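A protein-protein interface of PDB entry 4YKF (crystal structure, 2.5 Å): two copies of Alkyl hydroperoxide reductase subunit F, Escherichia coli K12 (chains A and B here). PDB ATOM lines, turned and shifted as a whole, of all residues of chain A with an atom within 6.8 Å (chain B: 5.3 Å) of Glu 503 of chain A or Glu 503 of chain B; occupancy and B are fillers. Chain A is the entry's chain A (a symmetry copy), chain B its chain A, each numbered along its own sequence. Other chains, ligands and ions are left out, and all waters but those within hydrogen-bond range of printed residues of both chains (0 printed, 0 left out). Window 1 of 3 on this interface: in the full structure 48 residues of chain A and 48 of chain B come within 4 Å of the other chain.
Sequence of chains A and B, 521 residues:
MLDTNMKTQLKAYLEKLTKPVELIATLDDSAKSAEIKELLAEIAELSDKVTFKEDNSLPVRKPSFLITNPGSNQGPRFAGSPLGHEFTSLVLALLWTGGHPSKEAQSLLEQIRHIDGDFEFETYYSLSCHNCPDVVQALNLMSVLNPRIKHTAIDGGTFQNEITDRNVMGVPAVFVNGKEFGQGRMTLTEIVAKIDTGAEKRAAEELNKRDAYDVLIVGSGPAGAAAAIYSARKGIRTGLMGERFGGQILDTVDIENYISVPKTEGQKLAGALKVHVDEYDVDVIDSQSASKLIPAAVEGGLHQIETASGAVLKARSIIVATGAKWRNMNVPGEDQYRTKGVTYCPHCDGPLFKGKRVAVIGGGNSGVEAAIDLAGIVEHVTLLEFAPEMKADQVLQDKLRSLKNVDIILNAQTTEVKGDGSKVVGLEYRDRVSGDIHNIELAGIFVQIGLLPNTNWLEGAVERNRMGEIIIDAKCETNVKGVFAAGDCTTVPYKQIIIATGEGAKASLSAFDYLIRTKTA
NZ of Lys 506 of chain A lies within salt-bridge range of OE2 of Glu 503 of chain B. The side-chain amino group (NZ) of Lys 506 of chain B lies within salt-bridge range of the side-chain carboxylate (OE2) of Glu 503 of chain A (3.5 Å).
The side-chain amino group (NZ) of Lys 506 of chain B is in salt-bridge range of the side-chain carboxylate (OE2) of Glu 503 of chain B, 3.1 Å away. The backbone carbonyl oxygen (O) of Glu 503 of chain A lies within hydrogen-bond range of the side-chain sulfur (SG) of Cys 476 of chain A (3.7 Å). The backbone carbonyl oxygen of Ile 498 of chain A is in hydrogen-bond range of the side-chain hydroxyl of Thr 501 of chain A (3.0 Å). OE2 of Glu 503 of chain A lies within salt-bridge range of NZ of Lys 506 of chain A, at 3.1 Å. SG of Cys 476 of chain B is in hydrogen-bond range of O of Glu 503 of chain B (3.7 Å).
Ile 498 of chain A touches Thr 501 of chain B (CG1 to OG1, 3.6 Å). O of Ile 498 of chain A touches CA of Gly 502 of chain B, 3.9 Å away. Ala 505 of chain B touches Ile 498 of chain A (CB to CG2, 3.9 Å). O of Gly 502 of chain B touches CG1 of Ile 499 of chain A (3.7 Å). Ala 505 of chain B touches Ile 499 of chain A. Ile 499 of chain A touches Lys 506 of chain B (CD1 to CG, 3.9 Å). O of Gly 502 of chain A touches CG1 of Ile 499 of chain B, at 3.7 Å. Glu 503 of chain A touches Glu 503 of chain B. Ala 505 of chain A touches Ile 499 of chain B (CB to CG1, 3.9 Å). Ile 499 of chain B touches Lys 506 of chain A (CD1 to CG, 3.9 Å).
Of the printed residues of chain B, Glu 503 of chain A touches Glu 503 and Lys 506. Glu 503 of chain B touches just these residues of chain A: Glu 503 (3.9 Å) and Lys 506 (3.5 Å). Of the printed residues of chain A, Lys 506 of chain B touches Ile 499 (3.9 Å) and Glu 503 (3.5 Å). Of the printed residues of chain A, Gly 502 of chain B touches Ile 498 (3.9 Å) and Ile 499 (3.7 Å). Printed residues of chain A within 4 Å of Ile 499 of chain B: Gly 502 (3.7 Å), Ala 505 (3.9 Å) and Lys 506 (3.9 Å). Printed residues of chain B within 4 Å of Gly 502 of chain A: Ile 499 (3.7 Å). The nearest printed residue of chain B that does not touch Glu 503 of chain A is Ile 499 of chain B (5.7 Å). The nearest printed residue of chain A that does not touch Ala 505 of chain B is Ala 500 of chain A (7.9 Å).
Hydrophobic or aromatic side chains of chain B that line the printed part of chain A: Ile 499 and Ala 505. Among the printed residues, 12 pairs touch across the chains.
Ile 499 of chain A touches Gly 502 of chain B, and with the chains exchanged Gly 502 of chain A touches Ile 499 of chain B. Ile 499 of chain A touches Lys 506 of chain B, and with the chains exchanged Lys 506 of chain A touches Ile 499 of chain B. Glu 503 of chain B touches its own counterpart, Glu 503 of chain A. Glu 503 of chain A touches Lys 506 of chain B, and with the chains exchanged Lys 506 of chain A touches Glu 503 of chain B. 17 positions are printed for both chains. Of the 12 pairs that touch across the chains among the printed residues, 9 have their exchanged pair printed and touching as well.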
ATOM      1  N   ALA A 223      -2.585  23.191  -4.703  1.00  0.00           N
ATOM      2  CA  ALA A 223      -3.288  22.111  -4.086  1.00  0.00           C
ATOM      3  C   ALA A 223      -2.341  21.029  -3.588  1.00  0.00           C
ATOM      4  O   ALA A 223      -2.444  20.586  -2.445  1.00  0.00           O
ATOM      5  CB  ALA A 223      -4.305  21.521  -5.056  1.00  0.00           C
ATOM      6  N   ALA A 226      -0.353  22.131  -0.449  1.00  0.00           N
ATOM      7  CA  ALA A 226      -1.118  22.211   0.740  1.00  0.00           C
ATOM      8  C   ALA A 226      -1.317  20.807   1.276  1.00  0.00           C
ATOM      9  O   ALA A 226      -1.156  20.533   2.485  1.00  0.00           O
ATOM     10  CB  ALA A 226      -2.440  22.843   0.438  1.00  0.00           C
ATOM     11  N   ALA A 227      -1.614  19.907   0.370  1.00  0.00           N
ATOM     12  CA  ALA A 227      -1.693  18.481   0.736  1.00  0.00           C
ATOM     13  C   ALA A 227      -0.455  18.001   1.386  1.00  0.00           C
ATOM     14  O   ALA A 227      -0.536  17.203   2.292  1.00  0.00           O
ATOM     15  CB  ALA A 227      -2.008  17.565  -0.464  1.00  0.00           C
ATOM     16  N   ILE A 319      -2.859  11.270  -3.858  1.00  0.00           N
ATOM     17  CA  ILE A 319      -3.654  12.427  -4.085  1.00  0.00           C
ATOM     18  C   ILE A 319      -3.245  13.041  -5.390  1.00  0.00           C
ATOM     19  O   ILE A 319      -2.105  13.438  -5.577  1.00  0.00           O
ATOM     20  CB  ILE A 319      -3.464  13.429  -2.977  1.00  0.00           C
ATOM     21  CG1 ILE A 319      -3.720  12.744  -1.644  1.00  0.00           C
ATOM     22  CG2 ILE A 319      -4.399  14.595  -3.189  1.00  0.00           C
ATOM     23  CD1 ILE A 319      -3.521  13.655  -0.455  1.00  0.00           C
ATOM     24  N   ILE A 472     -15.245  13.904  -7.305  1.00  0.00           N
ATOM     25  CA  ILE A 472     -14.983  13.718  -5.889  1.00  0.00           C
ATOM     26  C   ILE A 472     -16.183  13.942  -5.003  1.00  0.00           C
ATOM     27  O   ILE A 472     -16.963  14.749  -5.289  1.00  0.00           O
ATOM     28  CB  ILE A 472     -13.832  14.606  -5.349  1.00  0.00           C
ATOM     29  CG1 ILE A 472     -14.086  16.099  -5.564  1.00  0.00           C
ATOM     30  CG2 ILE A 472     -12.507  14.132  -5.930  1.00  0.00           C
ATOM     31  CD1 ILE A 472     -13.009  16.966  -4.974  1.00  0.00           C
ATOM     32  N   ASP A 473     -16.300  13.219  -3.912  1.00  0.00           N
ATOM     33  CA  ASP A 473     -17.260  13.605  -2.872  1.00  0.00           C
ATOM     34  C   ASP A 473     -16.622  14.683  -1.994  1.00  0.00           C
ATOM     35  O   ASP A 473     -15.517  15.139  -2.281  1.00  0.00           O
ATOM     36  CB  ASP A 473     -17.670  12.401  -2.054  1.00  0.00           C
ATOM     37  CG  ASP A 473     -16.543  11.826  -1.306  1.00  0.00           C
ATOM     38  OD1 ASP A 473     -15.538  12.572  -1.079  1.00  0.00           O
ATOM     39  OD2 ASP A 473     -16.664  10.630  -0.958  1.00  0.00           O
ATOM     40  N   ALA A 474     -17.305  15.089  -0.933  1.00  0.00           N
ATOM     41  CA  ALA A 474     -16.920  16.272  -0.136  1.00  0.00           C
ATOM     42  C   ALA A 474     -15.625  16.036   0.530  1.00  0.00           C
ATOM     43  O   ALA A 474     -14.948  16.987   0.840  1.00  0.00           O
ATOM     44  CB  ALA A 474     -17.952  16.596   0.927  1.00  0.00           C
ATOM     45  N   LYS A 475     -15.301  14.759   0.721  1.00  0.00           N
ATOM     46  CA  LYS A 475     -14.078  14.288   1.397  1.00  0.00           C
ATOM     47  C   LYS A 475     -12.919  14.110   0.432  1.00  0.00           C
ATOM     48  O   LYS A 475     -11.849  13.552   0.828  1.00  0.00           O
ATOM     49  CB  LYS A 475     -14.344  12.934   2.105  1.00  0.00           C
ATOM     50  CG  LYS A 475     -14.759  13.037   3.578  1.00  0.00           C
ATOM     51  CD  LYS A 475     -14.986  11.679   4.286  1.00  0.00           C
ATOM     52  CE  LYS A 475     -13.669  10.940   4.670  1.00  0.00           C
ATOM     53  NZ  LYS A 475     -13.173  11.171   6.098  1.00  0.00           N
ATOM     54  N   CYS A 476     -13.149  14.533  -0.827  1.00  0.00           N
ATOM     55  CA  CYS A 476     -12.166  14.427  -1.901  1.00  0.00           C
ATOM     56  C   CYS A 476     -11.886  12.996  -2.379  1.00  0.00           C
ATOM     57  O   CYS A 476     -10.872  12.742  -3.008  1.00  0.00           O
ATOM     58  CB  CYS A 476     -10.856  15.136  -1.504  1.00  0.00           C
ATOM     59  SG  CYS A 476     -11.027  16.943  -1.384  1.00  0.00           S
ATOM     60  N   ALA A 485      -8.326  13.249  -4.805  1.00  0.00           N
ATOM     61  CA  ALA A 485      -7.998  14.288  -5.722  1.00  0.00           C
ATOM     62  C   ALA A 485      -8.365  15.674  -5.124  1.00  0.00           C
ATOM     63  O   ALA A 485      -9.310  15.787  -4.379  1.00  0.00           O
ATOM     64  CB  ALA A 485      -8.772  14.079  -7.048  1.00  0.00           C
ATOM     65  N   ALA A 486      -7.610  16.700  -5.511  1.00  0.00           N
ATOM     66  CA  ALA A 486      -7.903  18.049  -5.122  1.00  0.00           C
ATOM     67  C   ALA A 486      -7.524  19.012  -6.190  1.00  0.00           C
ATOM     68  O   ALA A 486      -6.584  18.771  -6.924  1.00  0.00           O
ATOM     69  CB  ALA A 486      -7.104  18.414  -3.897  1.00  0.00           C
ATOM     70  N   GLY A 487      -8.244  20.119  -6.214  1.00  0.00           N
ATOM     71  CA  GLY A 487      -7.911  21.235  -6.994  1.00  0.00           C
ATOM     72  C   GLY A 487      -8.607  21.319  -8.325  1.00  0.00           C
ATOM     73  O   GLY A 487      -9.620  20.689  -8.533  1.00  0.00           O
ATOM     74  N   ASP A 488      -8.074  22.146  -9.202  1.00  0.00           N
ATOM     75  CA  ASP A 488      -8.721  22.425 -10.514  1.00  0.00           C
ATOM     76  C   ASP A 488      -8.981  21.179 -11.347  1.00  0.00           C
ATOM     77  O   ASP A 488      -9.903  21.190 -12.163  1.00  0.00           O
ATOM     78  CB  ASP A 488      -7.876  23.420 -11.347  1.00  0.00           C
ATOM     79  CG  ASP A 488      -7.872  24.837 -10.759  1.00  0.00           C
ATOM     80  OD1 ASP A 488      -8.469  25.046  -9.660  1.00  0.00           O
ATOM     81  OD2 ASP A 488      -7.227  25.740 -11.347  1.00  0.00           O
ATOM     82  N   THR A 490     -10.393  18.498 -10.437  1.00  0.00           N
ATOM     83  CA  THR A 490     -11.580  17.823  -9.950  1.00  0.00           C
ATOM     84  C   THR A 490     -12.861  18.529 -10.302  1.00  0.00           C
ATOM     85  O   THR A 490     -12.839  19.572 -10.930  1.00  0.00           O
ATOM     86  CB  THR A 490     -11.526  17.660  -8.380  1.00  0.00           C
ATOM     87  OG1 THR A 490     -11.903  18.894  -7.723  1.00  0.00           O
ATOM     88  CG2 THR A 490     -10.168  17.290  -7.985  1.00  0.00           C
ATOM     89  N   VAL A 492     -14.640  20.197  -8.323  1.00  0.00           N
ATOM     90  CA  VAL A 492     -14.812  21.392  -7.615  1.00  0.00           C
ATOM     91  C   VAL A 492     -15.286  22.485  -8.606  1.00  0.00           C
ATOM     92  O   VAL A 492     -14.611  22.791  -9.582  1.00  0.00           O
ATOM     93  CB  VAL A 492     -13.486  21.789  -6.917  1.00  0.00           C
ATOM     94  CG1 VAL A 492     -12.417  22.232  -7.949  1.00  0.00           C
ATOM     95  CG2 VAL A 492     -13.729  22.862  -5.885  1.00  0.00           C
ATOM     96  N   ILE A 498      -7.063  29.916  -3.485  1.00  0.00           N
ATOM     97  CA  ILE A 498      -7.454  29.728  -2.095  1.00  0.00           C
ATOM     98  C   ILE A 498      -8.377  28.514  -1.991  1.00  0.00           C
ATOM     99  O   ILE A 498      -8.256  27.724  -1.064  1.00  0.00           O
ATOM    100  CB  ILE A 498      -7.989  31.032  -1.475  1.00  0.00           C
ATOM    101  CG1 ILE A 498      -8.058  30.960   0.077  1.00  0.00           C
ATOM    102  CG2 ILE A 498      -9.356  31.319  -2.003  1.00  0.00           C
ATOM    103  CD1 ILE A 498      -6.796  31.308   0.831  1.00  0.00           C
ATOM    104  N   ILE A 499      -9.184  28.273  -3.025  1.00  0.00           N
ATOM    105  CA  ILE A 499     -10.025  27.095  -3.075  1.00  0.00           C
ATOM    106  C   ILE A 499      -9.149  25.889  -3.287  1.00  0.00           C
ATOM    107  O   ILE A 499      -9.286  24.890  -2.585  1.00  0.00           O
ATOM    108  CB  ILE A 499     -11.038  27.228  -4.181  1.00  0.00           C
ATOM    109  CG1 ILE A 499     -11.949  28.426  -3.899  1.00  0.00           C
ATOM    110  CG2 ILE A 499     -11.892  25.962  -4.307  1.00  0.00           C
ATOM    111  CD1 ILE A 499     -12.734  28.912  -5.085  1.00  0.00           C
ATOM    112  N   ALA A 500      -8.192  25.972  -4.224  1.00  0.00           N
ATOM    113  CA  ALA A 500      -7.274  24.864  -4.432  1.00  0.00           C
ATOM    114  C   ALA A 500      -6.578  24.503  -3.125  1.00  0.00           C
ATOM    115  O   ALA A 500      -6.565  23.364  -2.770  1.00  0.00           O
ATOM    116  CB  ALA A 500      -6.269  25.208  -5.491  1.00  0.00           C
ATOM    117  N   THR A 501      -5.998  25.443  -2.390  1.00  0.00           N
ATOM    118  CA  THR A 501      -5.293  25.015  -1.188  1.00  0.00           C
ATOM    119  C   THR A 501      -6.236  24.334  -0.203  1.00  0.00           C
ATOM    120  O   THR A 501      -5.882  23.403   0.462  1.00  0.00           O
ATOM    121  CB  THR A 501      -4.547  26.121  -0.461  1.00  0.00           C
ATOM    122  OG1 THR A 501      -5.356  27.293  -0.406  1.00  0.00           O
ATOM    123  CG2 THR A 501      -3.400  26.468  -1.181  1.00  0.00           C
ATOM    124  N   GLY A 502      -7.454  24.777  -0.112  1.00  0.00           N
ATOM    125  CA  GLY A 502      -8.357  24.181   0.833  1.00  0.00           C
ATOM    126  C   GLY A 502      -8.595  22.731   0.537  1.00  0.00           C
ATOM    127  O   GLY A 502      -8.582  21.908   1.436  1.00  0.00           O
ATOM    128  N   GLU A 503      -8.826  22.426  -0.725  1.00  0.00           N
ATOM    129  CA  GLU A 503      -9.124  21.062  -1.153  1.00  0.00           C
ATOM    130  C   GLU A 503      -7.925  20.177  -0.895  1.00  0.00           C
ATOM    131  O   GLU A 503      -8.051  18.990  -0.551  1.00  0.00           O
ATOM    132  CB  GLU A 503      -9.435  21.036  -2.659  1.00  0.00           C
ATOM    133  CG  GLU A 503     -10.635  21.867  -3.040  1.00  0.00           C
ATOM    134  CD  GLU A 503     -11.984  21.376  -2.500  1.00  0.00           C
ATOM    135  OE1 GLU A 503     -12.354  20.188  -2.789  1.00  0.00           O
ATOM    136  OE2 GLU A 503     -12.738  22.228  -1.882  1.00  0.00           O
ATOM    137  N   GLY A 504      -6.760  20.758  -1.125  1.00  0.00           N
ATOM    138  CA  GLY A 504      -5.541  20.066  -0.870  1.00  0.00           C
ATOM    139  C   GLY A 504      -5.545  19.646   0.567  1.00  0.00           C
ATOM    140  O   GLY A 504      -5.358  18.502   0.849  1.00  0.00           O
ATOM    141  N   ALA A 505      -5.805  20.569   1.475  1.00  0.00           N
ATOM    142  CA  ALA A 505      -5.769  20.237   2.886  1.00  0.00           C
ATOM    143  C   ALA A 505      -6.754  19.139   3.193  1.00  0.00           C
ATOM    144  O   ALA A 505      -6.448  18.212   3.928  1.00  0.00           O
ATOM    145  CB  ALA A 505      -6.053  21.468   3.714  1.00  0.00           C
ATOM    146  N   LYS A 506      -7.960  19.287   2.665  1.00  0.00           N
ATOM    147  CA  LYS A 506      -9.017  18.257   2.832  1.00  0.00           C
ATOM    148  C   LYS A 506      -8.608  16.880   2.324  1.00  0.00           C
ATOM    149  O   LYS A 506      -8.741  15.888   3.040  1.00  0.00           O
ATOM    150  CB  LYS A 506     -10.268  18.656   2.107  1.00  0.00           C
ATOM    151  CG  LYS A 506     -10.997  19.760   2.804  1.00  0.00           C
ATOM    152  CD  LYS A 506     -12.443  19.807   2.363  1.00  0.00           C
ATOM    153  CE  LYS A 506     -12.606  20.835   1.263  1.00  0.00           C
ATOM    154  NZ  LYS A 506     -13.712  20.418   0.398  1.00  0.00           N
ATOM    155  N   ALA A 507      -8.092  16.831   1.114  1.00  0.00           N
ATOM    156  CA  ALA A 507      -7.697  15.564   0.530  1.00  0.00           C
ATOM    157  C   ALA A 507      -6.734  14.849   1.433  1.00  0.00           C
ATOM    158  O   ALA A 507      -6.839  13.628   1.603  1.00  0.00           O
ATOM    159  CB  ALA A 507      -7.079  15.752  -0.866  1.00  0.00           C
ATOM    160  N   SER A 508      -5.797  15.594   2.002  1.00  0.00           N
ATOM    161  CA  SER A 508      -4.764  15.031   2.882  1.00  0.00           C
ATOM    162  C   SER A 508      -5.298  14.451   4.196  1.00  0.00           C
ATOM    163  O   SER A 508      -4.961  13.357   4.606  1.00  0.00           O
ATOM    164  CB  SER A 508      -3.728  16.095   3.141  1.00  0.00           C
ATOM    165  OG  SER A 508      -2.982  15.837   4.278  1.00  0.00           O
ATOM    166  N   ILE B 472     -24.606  21.173   2.942  1.00  0.00           N
ATOM    167  CA  ILE B 472     -24.318  21.843   1.686  1.00  0.00           C
ATOM    168  C   ILE B 472     -23.922  20.914   0.566  1.00  0.00           C
ATOM    169  O   ILE B 472     -23.309  19.960   0.804  1.00  0.00           O
ATOM    170  CB  ILE B 472     -23.218  22.931   1.801  1.00  0.00           C
ATOM    171  CG1 ILE B 472     -21.892  22.378   2.328  1.00  0.00           C
ATOM    172  CG2 ILE B 472     -23.745  24.104   2.613  1.00  0.00           C
ATOM    173  CD1 ILE B 472     -20.803  23.413   2.367  1.00  0.00           C
ATOM    174  N   CYS B 476     -21.815  24.834  -2.115  1.00  0.00           N
ATOM    175  CA  CYS B 476     -22.176  25.486  -0.860  1.00  0.00           C
ATOM    176  C   CYS B 476     -23.659  25.862  -0.731  1.00  0.00           C
ATOM    177  O   CYS B 476     -24.017  26.691   0.088  1.00  0.00           O
ATOM    178  CB  CYS B 476     -21.279  26.715  -0.614  1.00  0.00           C
ATOM    179  SG  CYS B 476     -19.544  26.280  -0.280  1.00  0.00           S
ATOM    180  N   ALA B 485     -23.901  28.520   2.659  1.00  0.00           N
ATOM    181  CA  ALA B 485     -23.180  28.403   3.881  1.00  0.00           C
ATOM    182  C   ALA B 485     -21.710  27.985   3.604  1.00  0.00           C
ATOM    183  O   ALA B 485     -21.443  27.277   2.662  1.00  0.00           O
ATOM    184  CB  ALA B 485     -23.854  27.340   4.786  1.00  0.00           C
ATOM    185  N   ALA B 486     -20.801  28.420   4.475  1.00  0.00           N
ATOM    186  CA  ALA B 486     -19.425  28.020   4.401  1.00  0.00           C
ATOM    187  C   ALA B 486     -18.819  27.922   5.756  1.00  0.00           C
ATOM    188  O   ALA B 486     -19.204  28.651   6.650  1.00  0.00           O
ATOM    189  CB  ALA B 486     -18.633  29.052   3.639  1.00  0.00           C
ATOM    190  N   GLY B 487     -17.835  27.047   5.856  1.00  0.00           N
ATOM    191  CA  GLY B 487     -16.997  26.958   6.977  1.00  0.00           C
ATOM    192  C   GLY B 487     -17.389  25.919   7.991  1.00  0.00           C
ATOM    193  O   GLY B 487     -18.130  25.010   7.689  1.00  0.00           O
ATOM    194  N   THR B 490     -20.862  24.125   8.574  1.00  0.00           N
ATOM    195  CA  THR B 490     -21.441  23.251   7.574  1.00  0.00           C
ATOM    196  C   THR B 490     -20.983  21.821   7.686  1.00  0.00           C
ATOM    197  O   THR B 490     -20.191  21.494   8.551  1.00  0.00           O
ATOM    198  CB  THR B 490     -21.098  23.761   6.119  1.00  0.00           C
ATOM    199  OG1 THR B 490     -19.754  23.377   5.743  1.00  0.00           O
ATOM    200  CG2 THR B 490     -21.218  25.218   6.084  1.00  0.00           C
ATOM    201  N   VAL B 492     -18.922  20.400   5.789  1.00  0.00           N
ATOM    202  CA  VAL B 492     -17.583  20.231   5.420  1.00  0.00           C
ATOM    203  C   VAL B 492     -16.897  19.324   6.473  1.00  0.00           C
ATOM    204  O   VAL B 492     -16.860  19.643   7.656  1.00  0.00           O
ATOM    205  CB  VAL B 492     -16.885  21.609   5.311  1.00  0.00           C
ATOM    206  CG1 VAL B 492     -16.706  22.262   6.706  1.00  0.00           C
ATOM    207  CG2 VAL B 492     -15.565  21.482   4.593  1.00  0.00           C
ATOM    208  N   ILE B 499      -9.193  25.654   4.907  1.00  0.00           N
ATOM    209  CA  ILE B 499     -10.389  25.044   4.365  1.00  0.00           C
ATOM    210  C   ILE B 499     -11.528  26.019   4.500  1.00  0.00           C
ATOM    211  O   ILE B 499     -12.264  26.252   3.544  1.00  0.00           O
ATOM    212  CB  ILE B 499     -10.689  23.759   5.089  1.00  0.00           C
ATOM    213  CG1 ILE B 499      -9.538  22.771   4.876  1.00  0.00           C
ATOM    214  CG2 ILE B 499     -11.993  23.130   4.587  1.00  0.00           C
ATOM    215  CD1 ILE B 499      -9.511  21.619   5.842  1.00  0.00           C
ATOM    216  N   ALA B 500     -11.668  26.652   5.675  1.00  0.00           N
ATOM    217  CA  ALA B 500     -12.710  27.652   5.847  1.00  0.00           C
ATOM    218  C   ALA B 500     -12.588  28.732   4.778  1.00  0.00           C
ATOM    219  O   ALA B 500     -13.554  29.034   4.146  1.00  0.00           O
ATOM    220  CB  ALA B 500     -12.638  28.254   7.219  1.00  0.00           C
ATOM    221  N   THR B 501     -11.422  29.324   4.551  1.00  0.00           N
ATOM    222  CA  THR B 501     -11.396  30.394   3.561  1.00  0.00           C
ATOM    223  C   THR B 501     -11.805  29.888   2.183  1.00  0.00           C
ATOM    224  O   THR B 501     -12.450  30.564   1.433  1.00  0.00           O
ATOM    225  CB  THR B 501     -10.062  31.113   3.438  1.00  0.00           C
ATOM    226  OG1 THR B 501      -8.999  30.164   3.458  1.00  0.00           O
ATOM    227  CG2 THR B 501      -9.870  31.941   4.549  1.00  0.00           C
ATOM    228  N   GLY B 502     -11.452  28.685   1.841  1.00  0.00           N
ATOM    229  CA  GLY B 502     -11.791  28.192   0.534  1.00  0.00           C
ATOM    230  C   GLY B 502     -13.274  28.131   0.329  1.00  0.00           C
ATOM    231  O   GLY B 502     -13.770  28.529  -0.710  1.00  0.00           O
ATOM    232  N   GLU B 503     -13.977  27.616   1.320  1.00  0.00           N
ATOM    233  CA  GLU B 503     -15.425  27.448   1.240  1.00  0.00           C
ATOM    234  C   GLU B 503     -16.088  28.803   1.138  1.00  0.00           C
ATOM    235  O   GLU B 503     -17.113  28.979   0.460  1.00  0.00           O
ATOM    236  CB  GLU B 503     -15.946  26.743   2.504  1.00  0.00           C
ATOM    237  CG  GLU B 503     -15.373  25.362   2.703  1.00  0.00           C
ATOM    238  CD  GLU B 503     -15.773  24.317   1.654  1.00  0.00           C
ATOM    239  OE1 GLU B 503     -17.017  24.088   1.474  1.00  0.00           O
ATOM    240  OE2 GLU B 503     -14.833  23.629   1.090  1.00  0.00           O
ATOM    241  N   GLY B 504     -15.519  29.744   1.872  1.00  0.00           N
ATOM    242  CA  GLY B 504     -15.999  31.085   1.833  1.00  0.00           C
ATOM    243  C   GLY B 504     -15.946  31.547   0.409  1.00  0.00           C
ATOM    244  O   GLY B 504     -16.925  31.996  -0.103  1.00  0.00           O
ATOM    245  N   ALA B 505     -14.808  31.395  -0.243  1.00  0.00           N
ATOM    246  CA  ALA B 505     -14.677  31.874  -1.606  1.00  0.00           C
ATOM    247  C   ALA B 505     -15.697  31.212  -2.496  1.00  0.00           C
ATOM    248  O   ALA B 505     -16.319  31.861  -3.323  1.00  0.00           O
ATOM    249  CB  ALA B 505     -13.274  31.625  -2.109  1.00  0.00           C
ATOM    250  N   LYS B 506     -15.817  29.900  -2.353  1.00  0.00           N
ATOM    251  CA  LYS B 506     -16.821  29.120  -3.120  1.00  0.00           C
ATOM    252  C   LYS B 506     -18.252  29.600  -2.909  1.00  0.00           C
ATOM    253  O   LYS B 506     -18.977  29.840  -3.875  1.00  0.00           O
ATOM    254  CB  LYS B 506     -16.769  27.670  -2.743  1.00  0.00           C
ATOM    255  CG  LYS B 506     -15.562  26.985  -3.302  1.00  0.00           C
ATOM    256  CD  LYS B 506     -15.770  25.487  -3.342  1.00  0.00           C
ATOM    257  CE  LYS B 506     -15.154  24.855  -2.110  1.00  0.00           C
ATOM    258  NZ  LYS B 506     -15.906  23.641  -1.785  1.00  0.00           N
ATOM    259  N   ALA B 507     -18.637  29.764  -1.661  1.00  0.00           N
ATOM    260  CA  ALA B 507     -19.989  30.192  -1.355  1.00  0.00           C
ATOM    261  C   ALA B 507     -20.307  31.473  -2.070  1.00  0.00           C
ATOM    262  O   ALA B 507     -21.418  31.627  -2.594  1.00  0.00           O
ATOM    263  CB  ALA B 507     -20.200  30.361   0.159  1.00  0.00           C
ATOM    264  N   SER B 508     -19.350  32.390  -2.089  1.00  0.00           N
ATOM    265  CA  SER B 508     -19.526  33.706  -2.720  1.00  0.00           C
ATOM    266  C   SER B 508     -19.705  33.660  -4.241  1.00  0.00           C
ATOM    267  O   SER B 508     -20.585  34.277  -4.809  1.00  0.00           O
ATOM    268  CB  SER B 508     -18.357  34.577  -2.338  1.00  0.00           C
ATOM    269  OG  SER B 508     -18.186  35.639  -3.208  1.00  0.00           O
